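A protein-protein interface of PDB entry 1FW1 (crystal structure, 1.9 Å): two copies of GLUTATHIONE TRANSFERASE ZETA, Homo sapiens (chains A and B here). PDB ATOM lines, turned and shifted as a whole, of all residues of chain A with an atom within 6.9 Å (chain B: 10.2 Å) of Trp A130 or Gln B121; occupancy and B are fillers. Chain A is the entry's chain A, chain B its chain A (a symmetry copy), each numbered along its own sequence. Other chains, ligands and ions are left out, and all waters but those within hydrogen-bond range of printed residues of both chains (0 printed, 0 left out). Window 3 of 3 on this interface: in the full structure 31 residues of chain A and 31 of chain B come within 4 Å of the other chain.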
ATOM      1  N   PRO A 112     -13.563  19.466 -28.288  1.00  0.00           N
ATOM      2  CA  PRO A 112     -12.772  19.783 -27.082  1.00  0.00           C
ATOM      3  C   PRO A 112     -13.051  18.863 -25.897  1.00  0.00           C
ATOM      4  O   PRO A 112     -12.136  18.541 -25.128  1.00  0.00           O
ATOM      5  CB  PRO A 112     -13.166  21.236 -26.779  1.00  0.00           C
ATOM      6  CG  PRO A 112     -13.384  21.798 -28.205  1.00  0.00           C
ATOM      7  CD  PRO A 112     -14.166  20.697 -28.862  1.00  0.00           C
ATOM      8  N   LEU A 113     -14.310  18.458 -25.737  1.00  0.00           N
ATOM      9  CA  LEU A 113     -14.651  17.591 -24.640  1.00  0.00           C
ATOM     10  C   LEU A 113     -14.163  16.149 -24.819  1.00  0.00           C
ATOM     11  O   LEU A 113     -14.121  15.411 -23.834  1.00  0.00           O
ATOM     12  CB  LEU A 113     -16.164  17.586 -24.410  1.00  0.00           C
ATOM     13  CG  LEU A 113     -16.791  18.966 -24.276  1.00  0.00           C
ATOM     14  CD1 LEU A 113     -18.329  18.816 -24.016  1.00  0.00           C
ATOM     15  CD2 LEU A 113     -16.120  19.694 -23.146  1.00  0.00           C
ATOM     16  N   GLN A 114     -13.810  15.729 -26.043  1.00  0.00           N
ATOM     17  CA  GLN A 114     -13.314  14.360 -26.243  1.00  0.00           C
ATOM     18  C   GLN A 114     -11.883  14.369 -26.738  1.00  0.00           C
ATOM     19  O   GLN A 114     -11.367  13.356 -27.229  1.00  0.00           O
ATOM     20  CB  GLN A 114     -14.195  13.549 -27.191  1.00  0.00           C
ATOM     21  CG  GLN A 114     -14.638  14.263 -28.453  1.00  0.00           C
ATOM     22  CD  GLN A 114     -13.876  13.879 -29.722  1.00  0.00           C
ATOM     23  OE1 GLN A 114     -14.415  14.035 -30.820  1.00  0.00           O
ATOM     24  NE2 GLN A 114     -12.601  13.419 -29.589  1.00  0.00           N
ATOM     25  N   ASN A 115     -11.251  15.522 -26.574  1.00  0.00           N
ATOM     26  CA  ASN A 115      -9.849  15.724 -26.939  1.00  0.00           C
ATOM     27  C   ASN A 115      -8.981  14.817 -26.041  1.00  0.00           C
ATOM     28  O   ASN A 115      -9.262  14.647 -24.848  1.00  0.00           O
ATOM     29  CB  ASN A 115      -9.505  17.204 -26.725  1.00  0.00           C
ATOM     30  CG  ASN A 115      -8.079  17.565 -27.172  1.00  0.00           C
ATOM     31  OD1 ASN A 115      -7.645  17.216 -28.257  1.00  0.00           O
ATOM     32  ND2 ASN A 115      -7.379  18.321 -26.341  1.00  0.00           N
ATOM     33  N   VAL A 118      -7.985  15.828 -22.537  1.00  0.00           N
ATOM     34  CA  VAL A 118      -9.086  15.893 -21.570  1.00  0.00           C
ATOM     35  C   VAL A 118      -9.408  14.432 -21.183  1.00  0.00           C
ATOM     36  O   VAL A 118      -9.596  14.103 -20.004  1.00  0.00           O
ATOM     37  CB  VAL A 118     -10.311  16.568 -22.194  1.00  0.00           C
ATOM     38  CG1 VAL A 118     -11.532  16.404 -21.299  1.00  0.00           C
ATOM     39  CG2 VAL A 118     -10.000  18.046 -22.412  1.00  0.00           C
ATOM     40  N   LEU A 119      -9.432  13.537 -22.163  1.00  0.00           N
ATOM     41  CA  LEU A 119      -9.714  12.137 -21.862  1.00  0.00           C
ATOM     42  C   LEU A 119      -8.658  11.557 -20.898  1.00  0.00           C
ATOM     43  O   LEU A 119      -8.990  10.747 -20.038  1.00  0.00           O
ATOM     44  CB  LEU A 119      -9.762  11.312 -23.147  1.00  0.00           C
ATOM     45  CG  LEU A 119     -10.847  11.695 -24.149  1.00  0.00           C
ATOM     46  CD1 LEU A 119     -10.757  10.730 -25.329  1.00  0.00           C
ATOM     47  CD2 LEU A 119     -12.254  11.638 -23.507  1.00  0.00           C
ATOM     48  N   VAL A 122      -9.620  12.385 -17.487  1.00  0.00           N
ATOM     49  CA  VAL A 122     -10.864  11.789 -17.028  1.00  0.00           C
ATOM     50  C   VAL A 122     -10.724  10.395 -16.426  1.00  0.00           C
ATOM     51  O   VAL A 122     -11.531  10.016 -15.586  1.00  0.00           O
ATOM     52  CB  VAL A 122     -11.927  11.822 -18.171  1.00  0.00           C
ATOM     53  CG1 VAL A 122     -12.970  10.704 -18.009  1.00  0.00           C
ATOM     54  CG2 VAL A 122     -12.616  13.194 -18.156  1.00  0.00           C
ATOM     55  N   GLU A 125     -11.647   4.380 -16.912  1.00  0.00           N
ATOM     56  CA  GLU A 125     -12.991   3.851 -16.708  1.00  0.00           C
ATOM     57  C   GLU A 125     -14.123   4.731 -17.184  1.00  0.00           C
ATOM     58  O   GLU A 125     -15.168   4.213 -17.592  1.00  0.00           O
ATOM     59  CB  GLU A 125     -13.216   3.493 -15.232  1.00  0.00           C
ATOM     60  CG  GLU A 125     -12.898   2.054 -14.978  1.00  0.00           C
ATOM     61  CD  GLU A 125     -12.753   1.704 -13.512  1.00  0.00           C
ATOM     62  OE1 GLU A 125     -13.692   1.994 -12.729  1.00  0.00           O
ATOM     63  OE2 GLU A 125     -11.680   1.116 -13.170  1.00  0.00           O
ATOM     64  N   MET A 126     -13.914   6.052 -17.150  1.00  0.00           N
ATOM     65  CA  MET A 126     -14.964   6.989 -17.553  1.00  0.00           C
ATOM     66  C   MET A 126     -14.837   7.562 -18.960  1.00  0.00           C
ATOM     67  O   MET A 126     -15.798   8.134 -19.457  1.00  0.00           O
ATOM     68  CB  MET A 126     -15.054   8.127 -16.529  1.00  0.00           C
ATOM     69  CG  MET A 126     -15.939   9.288 -16.933  1.00  0.00           C
ATOM     70  SD  MET A 126     -17.725   8.957 -16.795  1.00  0.00           S
ATOM     71  CE  MET A 126     -17.772   8.331 -15.083  1.00  0.00           C
ATOM     72  N   GLN A 127     -13.675   7.376 -19.597  1.00  0.00           N
ATOM     73  CA  GLN A 127     -13.368   7.911 -20.936  1.00  0.00           C
ATOM     74  C   GLN A 127     -14.393   7.652 -22.029  1.00  0.00           C
ATOM     75  O   GLN A 127     -14.859   8.590 -22.697  1.00  0.00           O
ATOM     76  CB  GLN A 127     -11.995   7.376 -21.461  1.00  0.00           C
ATOM     77  CG  GLN A 127     -10.768   8.057 -20.827  1.00  0.00           C
ATOM     78  CD  GLN A 127      -9.405   7.443 -21.276  1.00  0.00           C
ATOM     79  OE1 GLN A 127      -9.325   6.788 -22.325  1.00  0.00           O
ATOM     80  NE2 GLN A 127      -8.334   7.679 -20.473  1.00  0.00           N
ATOM     81  N   LEU A 128     -14.697   6.382 -22.244  1.00  0.00           N
ATOM     82  CA  LEU A 128     -15.614   6.033 -23.299  1.00  0.00           C
ATOM     83  C   LEU A 128     -16.943   6.722 -23.100  1.00  0.00           C
ATOM     84  O   LEU A 128     -17.475   7.341 -24.022  1.00  0.00           O
ATOM     85  CB  LEU A 128     -15.794   4.518 -23.392  1.00  0.00           C
ATOM     86  CG  LEU A 128     -16.821   4.210 -24.495  1.00  0.00           C
ATOM     87  CD1 LEU A 128     -16.193   4.557 -25.864  1.00  0.00           C
ATOM     88  CD2 LEU A 128     -17.270   2.753 -24.441  1.00  0.00           C
ATOM     89  N   THR A 129     -17.456   6.655 -21.887  1.00  0.00           N
ATOM     90  CA  THR A 129     -18.740   7.280 -21.548  1.00  0.00           C
ATOM     91  C   THR A 129     -18.673   8.819 -21.697  1.00  0.00           C
ATOM     92  O   THR A 129     -19.618   9.458 -22.134  1.00  0.00           O
ATOM     93  CB  THR A 129     -19.130   6.900 -20.085  1.00  0.00           C
ATOM     94  OG1 THR A 129     -19.299   5.477 -20.007  1.00  0.00           O
ATOM     95  CG2 THR A 129     -20.427   7.598 -19.639  1.00  0.00           C
ATOM     96  N   TRP A 130     -17.549   9.414 -21.320  1.00  0.00           N
ATOM     97  CA  TRP A 130     -17.394  10.867 -21.409  1.00  0.00           C
ATOM     98  C   TRP A 130     -17.428  11.294 -22.879  1.00  0.00           C
ATOM     99  O   TRP A 130     -18.159  12.220 -23.257  1.00  0.00           O
ATOM    100  CB  TRP A 130     -16.069  11.268 -20.746  1.00  0.00           C
ATOM    101  CG  TRP A 130     -15.761  12.740 -20.723  1.00  0.00           C
ATOM    102  CD1 TRP A 130     -15.251  13.494 -21.742  1.00  0.00           C
ATOM    103  CD2 TRP A 130     -15.854  13.619 -19.585  1.00  0.00           C
ATOM    104  NE1 TRP A 130     -15.010  14.778 -21.310  1.00  0.00           N
ATOM    105  CE2 TRP A 130     -15.366  14.884 -19.995  1.00  0.00           C
ATOM    106  CE3 TRP A 130     -16.294  13.450 -18.265  1.00  0.00           C
ATOM    107  CZ2 TRP A 130     -15.302  15.982 -19.127  1.00  0.00           C
ATOM    108  CZ3 TRP A 130     -16.232  14.533 -17.400  1.00  0.00           C
ATOM    109  CH2 TRP A 130     -15.737  15.790 -17.835  1.00  0.00           C
ATOM    110  N   ALA A 131     -16.630  10.620 -23.703  1.00  0.00           N
ATOM    111  CA  ALA A 131     -16.566  10.938 -25.128  1.00  0.00           C
ATOM    112  C   ALA A 131     -17.904  10.695 -25.805  1.00  0.00           C
ATOM    113  O   ALA A 131     -18.321  11.488 -26.644  1.00  0.00           O
ATOM    114  CB  ALA A 131     -15.486  10.113 -25.809  1.00  0.00           C
ATOM    115  N   GLN A 132     -18.575   9.602 -25.447  1.00  0.00           N
ATOM    116  CA  GLN A 132     -19.849   9.271 -26.040  1.00  0.00           C
ATOM    117  C   GLN A 132     -20.922  10.310 -25.741  1.00  0.00           C
ATOM    118  O   GLN A 132     -21.726  10.657 -26.642  1.00  0.00           O
ATOM    119  CB  GLN A 132     -20.348   7.868 -25.579  1.00  0.00           C
ATOM    120  CG  GLN A 132     -19.601   6.700 -26.236  1.00  0.00           C
ATOM    121  CD  GLN A 132     -20.165   5.318 -25.881  1.00  0.00           C
ATOM    122  OE1 GLN A 132     -20.024   4.356 -26.661  1.00  0.00           O
ATOM    123  NE2 GLN A 132     -20.784   5.208 -24.718  1.00  0.00           N
ATOM    124  N   ASN A 133     -20.946  10.802 -24.501  1.00  0.00           N
ATOM    125  CA  ASN A 133     -21.966  11.769 -24.123  1.00  0.00           C
ATOM    126  C   ASN A 133     -21.700  13.140 -24.752  1.00  0.00           C
ATOM    127  O   ASN A 133     -22.671  13.871 -25.041  1.00  0.00           O
ATOM    128  CB  ASN A 133     -22.075  11.938 -22.610  1.00  0.00           C
ATOM    129  CG  ASN A 133     -22.356  10.644 -21.891  1.00  0.00           C
ATOM    130  OD1 ASN A 133     -23.098   9.741 -22.375  1.00  0.00           O
ATOM    131  ND2 ASN A 133     -21.772  10.533 -20.693  1.00  0.00           N
ATOM    132  N   ALA A 134     -20.410  13.501 -24.910  1.00  0.00           N
ATOM    133  CA  ALA A 134     -20.064  14.778 -25.553  1.00  0.00           C
ATOM    134  C   ALA A 134     -20.576  14.679 -26.994  1.00  0.00           C
ATOM    135  O   ALA A 134     -21.195  15.607 -27.518  1.00  0.00           O
ATOM    136  CB  ALA A 134     -18.532  15.015 -25.584  1.00  0.00           C
ATOM    137  N   ILE A 135     -20.324  13.550 -27.640  1.00  0.00           N
ATOM    138  CA  ILE A 135     -20.783  13.410 -29.008  1.00  0.00           C
ATOM    139  C   ILE A 135     -22.303  13.258 -29.169  1.00  0.00           C
ATOM    140  O   ILE A 135     -22.874  13.905 -30.025  1.00  0.00           O
ATOM    141  CB  ILE A 135     -20.087  12.275 -29.704  1.00  0.00           C
ATOM    142  CG1 ILE A 135     -18.580  12.570 -29.743  1.00  0.00           C
ATOM    143  CG2 ILE A 135     -20.679  12.090 -31.069  1.00  0.00           C
ATOM    144  CD1 ILE A 135     -17.730  11.488 -30.382  1.00  0.00           C
ATOM    145  N   PHE B  46     -32.366  24.187 -19.639  1.00  0.00           N
ATOM    146  CA  PHE B  46     -32.887  22.837 -19.832  1.00  0.00           C
ATOM    147  C   PHE B  46     -34.419  22.784 -19.915  1.00  0.00           C
ATOM    148  O   PHE B  46     -35.006  21.741 -20.218  1.00  0.00           O
ATOM    149  CB  PHE B  46     -32.379  21.935 -18.706  1.00  0.00           C
ATOM    150  CG  PHE B  46     -30.895  21.755 -18.711  1.00  0.00           C
ATOM    151  CD1 PHE B  46     -30.129  22.194 -17.645  1.00  0.00           C
ATOM    152  CD2 PHE B  46     -30.258  21.182 -19.800  1.00  0.00           C
ATOM    153  CE1 PHE B  46     -28.745  22.074 -17.654  1.00  0.00           C
ATOM    154  CE2 PHE B  46     -28.863  21.056 -19.823  1.00  0.00           C
ATOM    155  CZ  PHE B  46     -28.109  21.505 -18.746  1.00  0.00           C
ATOM    156  N   PRO B 112     -14.668  26.014 -23.059  1.00  0.00           N
ATOM    157  CA  PRO B 112     -15.391  24.727 -23.036  1.00  0.00           C
ATOM    158  C   PRO B 112     -14.984  23.806 -21.889  1.00  0.00           C
ATOM    159  O   PRO B 112     -15.826  23.087 -21.338  1.00  0.00           O
ATOM    160  CB  PRO B 112     -15.056  24.114 -24.404  1.00  0.00           C
ATOM    161  CG  PRO B 112     -14.965  25.378 -25.292  1.00  0.00           C
ATOM    162  CD  PRO B 112     -14.171  26.315 -24.427  1.00  0.00           C
ATOM    163  N   LEU B 113     -13.697  23.813 -21.544  1.00  0.00           N
ATOM    164  CA  LEU B 113     -13.238  22.969 -20.474  1.00  0.00           C
ATOM    165  C   LEU B 113     -13.658  23.453 -19.081  1.00  0.00           C
ATOM    166  O   LEU B 113     -13.594  22.668 -18.136  1.00  0.00           O
ATOM    167  CB  LEU B 113     -11.714  22.827 -20.517  1.00  0.00           C
ATOM    168  CG  LEU B 113     -11.154  22.408 -21.869  1.00  0.00           C
ATOM    169  CD1 LEU B 113      -9.596  22.272 -21.768  1.00  0.00           C
ATOM    170  CD2 LEU B 113     -11.785  21.105 -22.271  1.00  0.00           C
ATOM    171  N   GLN B 114     -14.071  24.722 -18.932  1.00  0.00           N
ATOM    172  CA  GLN B 114     -14.506  25.209 -17.615  1.00  0.00           C
ATOM    173  C   GLN B 114     -15.965  25.612 -17.641  1.00  0.00           C
ATOM    174  O   GLN B 114     -16.458  26.297 -16.736  1.00  0.00           O
ATOM    175  CB  GLN B 114     -13.648  26.366 -17.105  1.00  0.00           C
ATOM    176  CG  GLN B 114     -13.331  27.448 -18.118  1.00  0.00           C
ATOM    177  CD  GLN B 114     -14.155  28.729 -17.986  1.00  0.00           C
ATOM    178  OE1 GLN B 114     -13.700  29.787 -18.427  1.00  0.00           O
ATOM    179  NE2 GLN B 114     -15.391  28.639 -17.424  1.00  0.00           N
ATOM    180  N   ASN B 115     -16.646  25.149 -18.680  1.00  0.00           N
ATOM    181  CA  ASN B 115     -18.078  25.382 -18.865  1.00  0.00           C
ATOM    182  C   ASN B 115     -18.833  24.675 -17.720  1.00  0.00           C
ATOM    183  O   ASN B 115     -18.463  23.571 -17.299  1.00  0.00           O
ATOM    184  CB  ASN B 115     -18.485  24.809 -20.230  1.00  0.00           C
ATOM    185  CG  ASN B 115     -19.955  25.083 -20.587  1.00  0.00           C
ATOM    186  OD1 ASN B 115     -20.441  26.195 -20.468  1.00  0.00           O
ATOM    187  ND2 ASN B 115     -20.636  24.062 -21.083  1.00  0.00           N
ATOM    188  N   LEU B 116     -19.888  25.315 -17.223  1.00  0.00           N
ATOM    189  CA  LEU B 116     -20.689  24.779 -16.125  1.00  0.00           C
ATOM    190  C   LEU B 116     -21.051  23.289 -16.242  1.00  0.00           C
ATOM    191  O   LEU B 116     -20.803  22.503 -15.318  1.00  0.00           O
ATOM    192  CB  LEU B 116     -21.992  25.613 -15.969  1.00  0.00           C
ATOM    193  CG  LEU B 116     -22.854  25.094 -14.815  1.00  0.00           C
ATOM    194  CD1 LEU B 116     -22.112  25.390 -13.506  1.00  0.00           C
ATOM    195  CD2 LEU B 116     -24.293  25.766 -14.826  1.00  0.00           C
ATOM    196  N   SER B 117     -21.613  22.882 -17.371  1.00  0.00           N
ATOM    197  CA  SER B 117     -22.019  21.490 -17.528  1.00  0.00           C
ATOM    198  C   SER B 117     -20.849  20.525 -17.497  1.00  0.00           C
ATOM    199  O   SER B 117     -21.028  19.352 -17.180  1.00  0.00           O
ATOM    200  CB  SER B 117     -22.844  21.308 -18.814  1.00  0.00           C
ATOM    201  OG  SER B 117     -22.027  21.372 -19.976  1.00  0.00           O
ATOM    202  N   VAL B 118     -19.642  20.984 -17.828  1.00  0.00           N
ATOM    203  CA  VAL B 118     -18.484  20.089 -17.743  1.00  0.00           C
ATOM    204  C   VAL B 118     -18.060  20.072 -16.257  1.00  0.00           C
ATOM    205  O   VAL B 118     -17.775  19.014 -15.679  1.00  0.00           O
ATOM    206  CB  VAL B 118     -17.341  20.602 -18.625  1.00  0.00           C
ATOM    207  CG1 VAL B 118     -16.056  19.836 -18.342  1.00  0.00           C
ATOM    208  CG2 VAL B 118     -17.745  20.452 -20.088  1.00  0.00           C
ATOM    209  N   LEU B 119     -18.054  21.234 -15.616  1.00  0.00           N
ATOM    210  CA  LEU B 119     -17.678  21.284 -14.205  1.00  0.00           C
ATOM    211  C   LEU B 119     -18.634  20.428 -13.349  1.00  0.00           C
ATOM    212  O   LEU B 119     -18.202  19.799 -12.388  1.00  0.00           O
ATOM    213  CB  LEU B 119     -17.673  22.726 -13.704  1.00  0.00           C
ATOM    214  CG  LEU B 119     -16.680  23.668 -14.380  1.00  0.00           C
ATOM    215  CD1 LEU B 119     -16.798  25.034 -13.708  1.00  0.00           C
ATOM    216  CD2 LEU B 119     -15.231  23.133 -14.272  1.00  0.00           C
ATOM    217  N   LYS B 120     -19.920  20.392 -13.710  1.00  0.00           N
ATOM    218  CA  LYS B 120     -20.874  19.564 -12.966  1.00  0.00           C
ATOM    219  C   LYS B 120     -20.468  18.094 -13.055  1.00  0.00           C
ATOM    220  O   LYS B 120     -20.580  17.372 -12.067  1.00  0.00           O
ATOM    221  CB  LYS B 120     -22.313  19.735 -13.498  1.00  0.00           C
ATOM    222  CG  LYS B 120     -23.057  20.980 -12.941  1.00  0.00           C
ATOM    223  CD  LYS B 120     -24.404  21.258 -13.707  1.00  0.00           C
ATOM    224  CE  LYS B 120     -25.173  22.478 -13.134  1.00  0.00           C
ATOM    225  NZ  LYS B 120     -26.363  22.917 -13.970  1.00  0.00           N
ATOM    226  N   GLN B 121     -19.987  17.655 -14.221  1.00  0.00           N
ATOM    227  CA  GLN B 121     -19.576  16.254 -14.406  1.00  0.00           C
ATOM    228  C   GLN B 121     -18.247  15.949 -13.765  1.00  0.00           C
ATOM    229  O   GLN B 121     -17.900  14.805 -13.584  1.00  0.00           O
ATOM    230  CB  GLN B 121     -19.464  15.862 -15.901  1.00  0.00           C
ATOM    231  CG  GLN B 121     -20.796  15.738 -16.640  1.00  0.00           C
ATOM    232  CD  GLN B 121     -21.855  14.995 -15.827  1.00  0.00           C
ATOM    233  OE1 GLN B 121     -21.671  13.818 -15.446  1.00  0.00           O
ATOM    234  NE2 GLN B 121     -22.976  15.678 -15.545  1.00  0.00           N
ATOM    235  N   VAL B 122     -17.489  16.973 -13.434  1.00  0.00           N
ATOM    236  CA  VAL B 122     -16.187  16.733 -12.833  1.00  0.00           C
ATOM    237  C   VAL B 122     -16.212  16.468 -11.332  1.00  0.00           C
ATOM    238  O   VAL B 122     -15.331  15.783 -10.825  1.00  0.00           O
ATOM    239  CB  VAL B 122     -15.207  17.892 -13.200  1.00  0.00           C
ATOM    240  CG1 VAL B 122     -14.098  18.052 -12.148  1.00  0.00           C
ATOM    241  CG2 VAL B 122     -14.593  17.593 -14.576  1.00  0.00           C
ATOM    242  N   GLY B 123     -17.213  16.970 -10.613  1.00  0.00           N
ATOM    243  CA  GLY B 123     -17.227  16.700  -9.175  1.00  0.00           C
ATOM    244  C   GLY B 123     -16.703  17.884  -8.373  1.00  0.00           C
ATOM    245  O   GLY B 123     -15.647  18.430  -8.698  1.00  0.00           O
ATOM    246  N   GLU B 124     -17.429  18.291  -7.338  1.00  0.00           N
ATOM    247  CA  GLU B 124     -17.012  19.457  -6.578  1.00  0.00           C
ATOM    248  C   GLU B 124     -15.547  19.507  -6.152  1.00  0.00           C
ATOM    249  O   GLU B 124     -14.923  20.548  -6.265  1.00  0.00           O
ATOM    250  CB  GLU B 124     -17.870  19.650  -5.327  1.00  0.00           C
ATOM    251  CG  GLU B 124     -17.578  21.015  -4.702  1.00  0.00           C
ATOM    252  CD  GLU B 124     -18.231  21.227  -3.343  1.00  0.00           C
ATOM    253  OE1 GLU B 124     -18.464  20.210  -2.643  1.00  0.00           O
ATOM    254  OE2 GLU B 124     -18.481  22.425  -2.969  1.00  0.00           O
ATOM    255  N   GLU B 125     -15.004  18.394  -5.667  1.00  0.00           N
ATOM    256  CA  GLU B 125     -13.623  18.392  -5.197  1.00  0.00           C
ATOM    257  C   GLU B 125     -12.574  18.708  -6.237  1.00  0.00           C
ATOM    258  O   GLU B 125     -11.534  19.281  -5.899  1.00  0.00           O
ATOM    259  CB  GLU B 125     -13.281  17.054  -4.525  1.00  0.00           C
ATOM    260  CG  GLU B 125     -13.504  17.128  -3.048  1.00  0.00           C
ATOM    261  CD  GLU B 125     -13.531  15.779  -2.361  1.00  0.00           C
ATOM    262  OE1 GLU B 125     -12.557  15.000  -2.526  1.00  0.00           O
ATOM    263  OE2 GLU B 125     -14.545  15.527  -1.640  1.00  0.00           O
ATOM    264  N   MET B 126     -12.851  18.356  -7.497  1.00  0.00           N
ATOM    265  CA  MET B 126     -11.882  18.583  -8.571  1.00  0.00           C
ATOM    266  C   MET B 126     -12.134  19.809  -9.443  1.00  0.00           C
ATOM    267  O   MET B 126     -11.241  20.209 -10.177  1.00  0.00           O
ATOM    268  CB  MET B 126     -11.784  17.328  -9.446  1.00  0.00           C
ATOM    269  CG  MET B 126     -10.992  17.496 -10.727  1.00  0.00           C
ATOM    270  SD  MET B 126      -9.185  17.535 -10.494  1.00  0.00           S
ATOM    271  CE  MET B 126      -8.989  16.022  -9.496  1.00  0.00           C
ATOM    272  N   GLN B 127     -13.325  20.409  -9.330  1.00  0.00           N
ATOM    273  CA  GLN B 127     -13.749  21.567 -10.137  1.00  0.00           C
ATOM    274  C   GLN B 127     -12.789  22.743 -10.206  1.00  0.00           C
ATOM    275  O   GLN B 127     -12.420  23.198 -11.302  1.00  0.00           O
ATOM    276  CB  GLN B 127     -15.125  22.129  -9.646  1.00  0.00           C
ATOM    277  CG  GLN B 127     -16.340  21.289 -10.078  1.00  0.00           C
ATOM    278  CD  GLN B 127     -17.696  21.795  -9.493  1.00  0.00           C
ATOM    279  OE1 GLN B 127     -17.812  22.963  -9.093  1.00  0.00           O
ATOM    280  NE2 GLN B 127     -18.722  20.904  -9.466  1.00  0.00           N
ATOM    281  N   TRP B 130      -9.690  21.811 -11.967  1.00  0.00           N
ATOM    282  CA  TRP B 130      -9.928  21.550 -13.387  1.00  0.00           C
ATOM    283  C   TRP B 130     -10.016  22.879 -14.142  1.00  0.00           C
ATOM    284  O   TRP B 130      -9.363  23.069 -15.177  1.00  0.00           O
ATOM    285  CB  TRP B 130     -11.225  20.742 -13.535  1.00  0.00           C
ATOM    286  CG  TRP B 130     -11.609  20.359 -14.937  1.00  0.00           C
ATOM    287  CD1 TRP B 130     -12.226  21.145 -15.870  1.00  0.00           C
ATOM    288  CD2 TRP B 130     -11.486  19.054 -15.536  1.00  0.00           C
ATOM    289  NE1 TRP B 130     -12.505  20.412 -17.001  1.00  0.00           N
ATOM    290  CE2 TRP B 130     -12.067  19.130 -16.825  1.00  0.00           C
ATOM    291  CE3 TRP B 130     -10.949  17.835 -15.097  1.00  0.00           C
ATOM    292  CZ2 TRP B 130     -12.130  18.027 -17.686  1.00  0.00           C
ATOM    293  CZ3 TRP B 130     -11.010  16.739 -15.945  1.00  0.00           C
ATOM    294  CH2 TRP B 130     -11.600  16.841 -17.233  1.00  0.00           C
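The backbone carbonyl oxygen (O) of Leu A113 lies within hydrogen-bond range of the indole nitrogen (NE1) of Trp A130 (2.7 Å).
The indole nitrogen (NE1) of Trp B130 lies within hydrogen-bond range of the backbone carbonyl oxygen (O) of Leu B113, at 2.8 Å.
Pro A112 touches Leu B113 (O to CD2, 3.9 Å).
Pro B112 touches Leu A113 (O to CD2, 3.9 Å).
Leu A113 touches Val B118 (CD2 to CG2, 3.5 Å).
Leu B113 touches Val A118.
Val A122 touches Trp B130 (CG2 to CH2, 3.9 Å).
Gln B121 touches Trp A130.
CH2 of Trp A130 touches CG2 of Val B122, at 3.9 Å.
Printed residues of chain B within 4 Å of Trp A130: Gln B121 and Val B122.
Gln B121 touches just one residue of chain A: Trp A130.
No residue of chain B comes within 4 Å of Thr A129.
Ala A131 touches none of the printed residues of chain B.
Of the printed residues of chain A, Val B122 touches Trp A130.
Of the printed residues of chain A, Trp B130 touches Val A122 (3.9 Å).
Of the printed residues of chain B, Pro A112 touches Leu B113 (3.9 Å).
Printed residues of chain B within 4 Å of Val A118: Leu B113 (3.5 Å).
The nearest printed residue of chain B that does not touch Trp A130 is Val B118 (4.005 Å).
The nearest printed residue of chain B that does not touch Val A118 is Trp B130 (4.01 Å).
Printed residues of chain A that touch a printed residue of chain B: Pro A112, Leu A113, Val A118, Val A122 and Trp A130.
Hydrophobic or aromatic side chains of chain A within 4 Å of the printed part of chain B: Leu A113, Val A118, Val A122 and Trp A130.
Of the 18 printed residues of chain B, 6 touch a printed residue of chain A.
Printed residues of chain B that touch a printed residue of chain A: Pro B112, Leu B113, Val B118, Gln B121, Val B122 and Trp B130.
Hydrophobic or aromatic side chains of chain B that line the printed part of chain A: Leu B113, Val B118, Val B122 and Trp B130.
Among the printed residues, 7 pairs touch across the chains.
Pro A112 touches Leu B113, and with the chains exchanged Leu A113 touches Pro B112.
Leu A113 touches Val B118, and with the chains exchanged Val A118 touches Leu B113.
Val A122 touches Trp B130, and with the chains exchanged Trp A130 touches Val B122.
11 positions are printed for both chains.
Of the 7 pairs that touch across the chains among the printed residues, 6 have their exchanged pair printed and touching as well.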
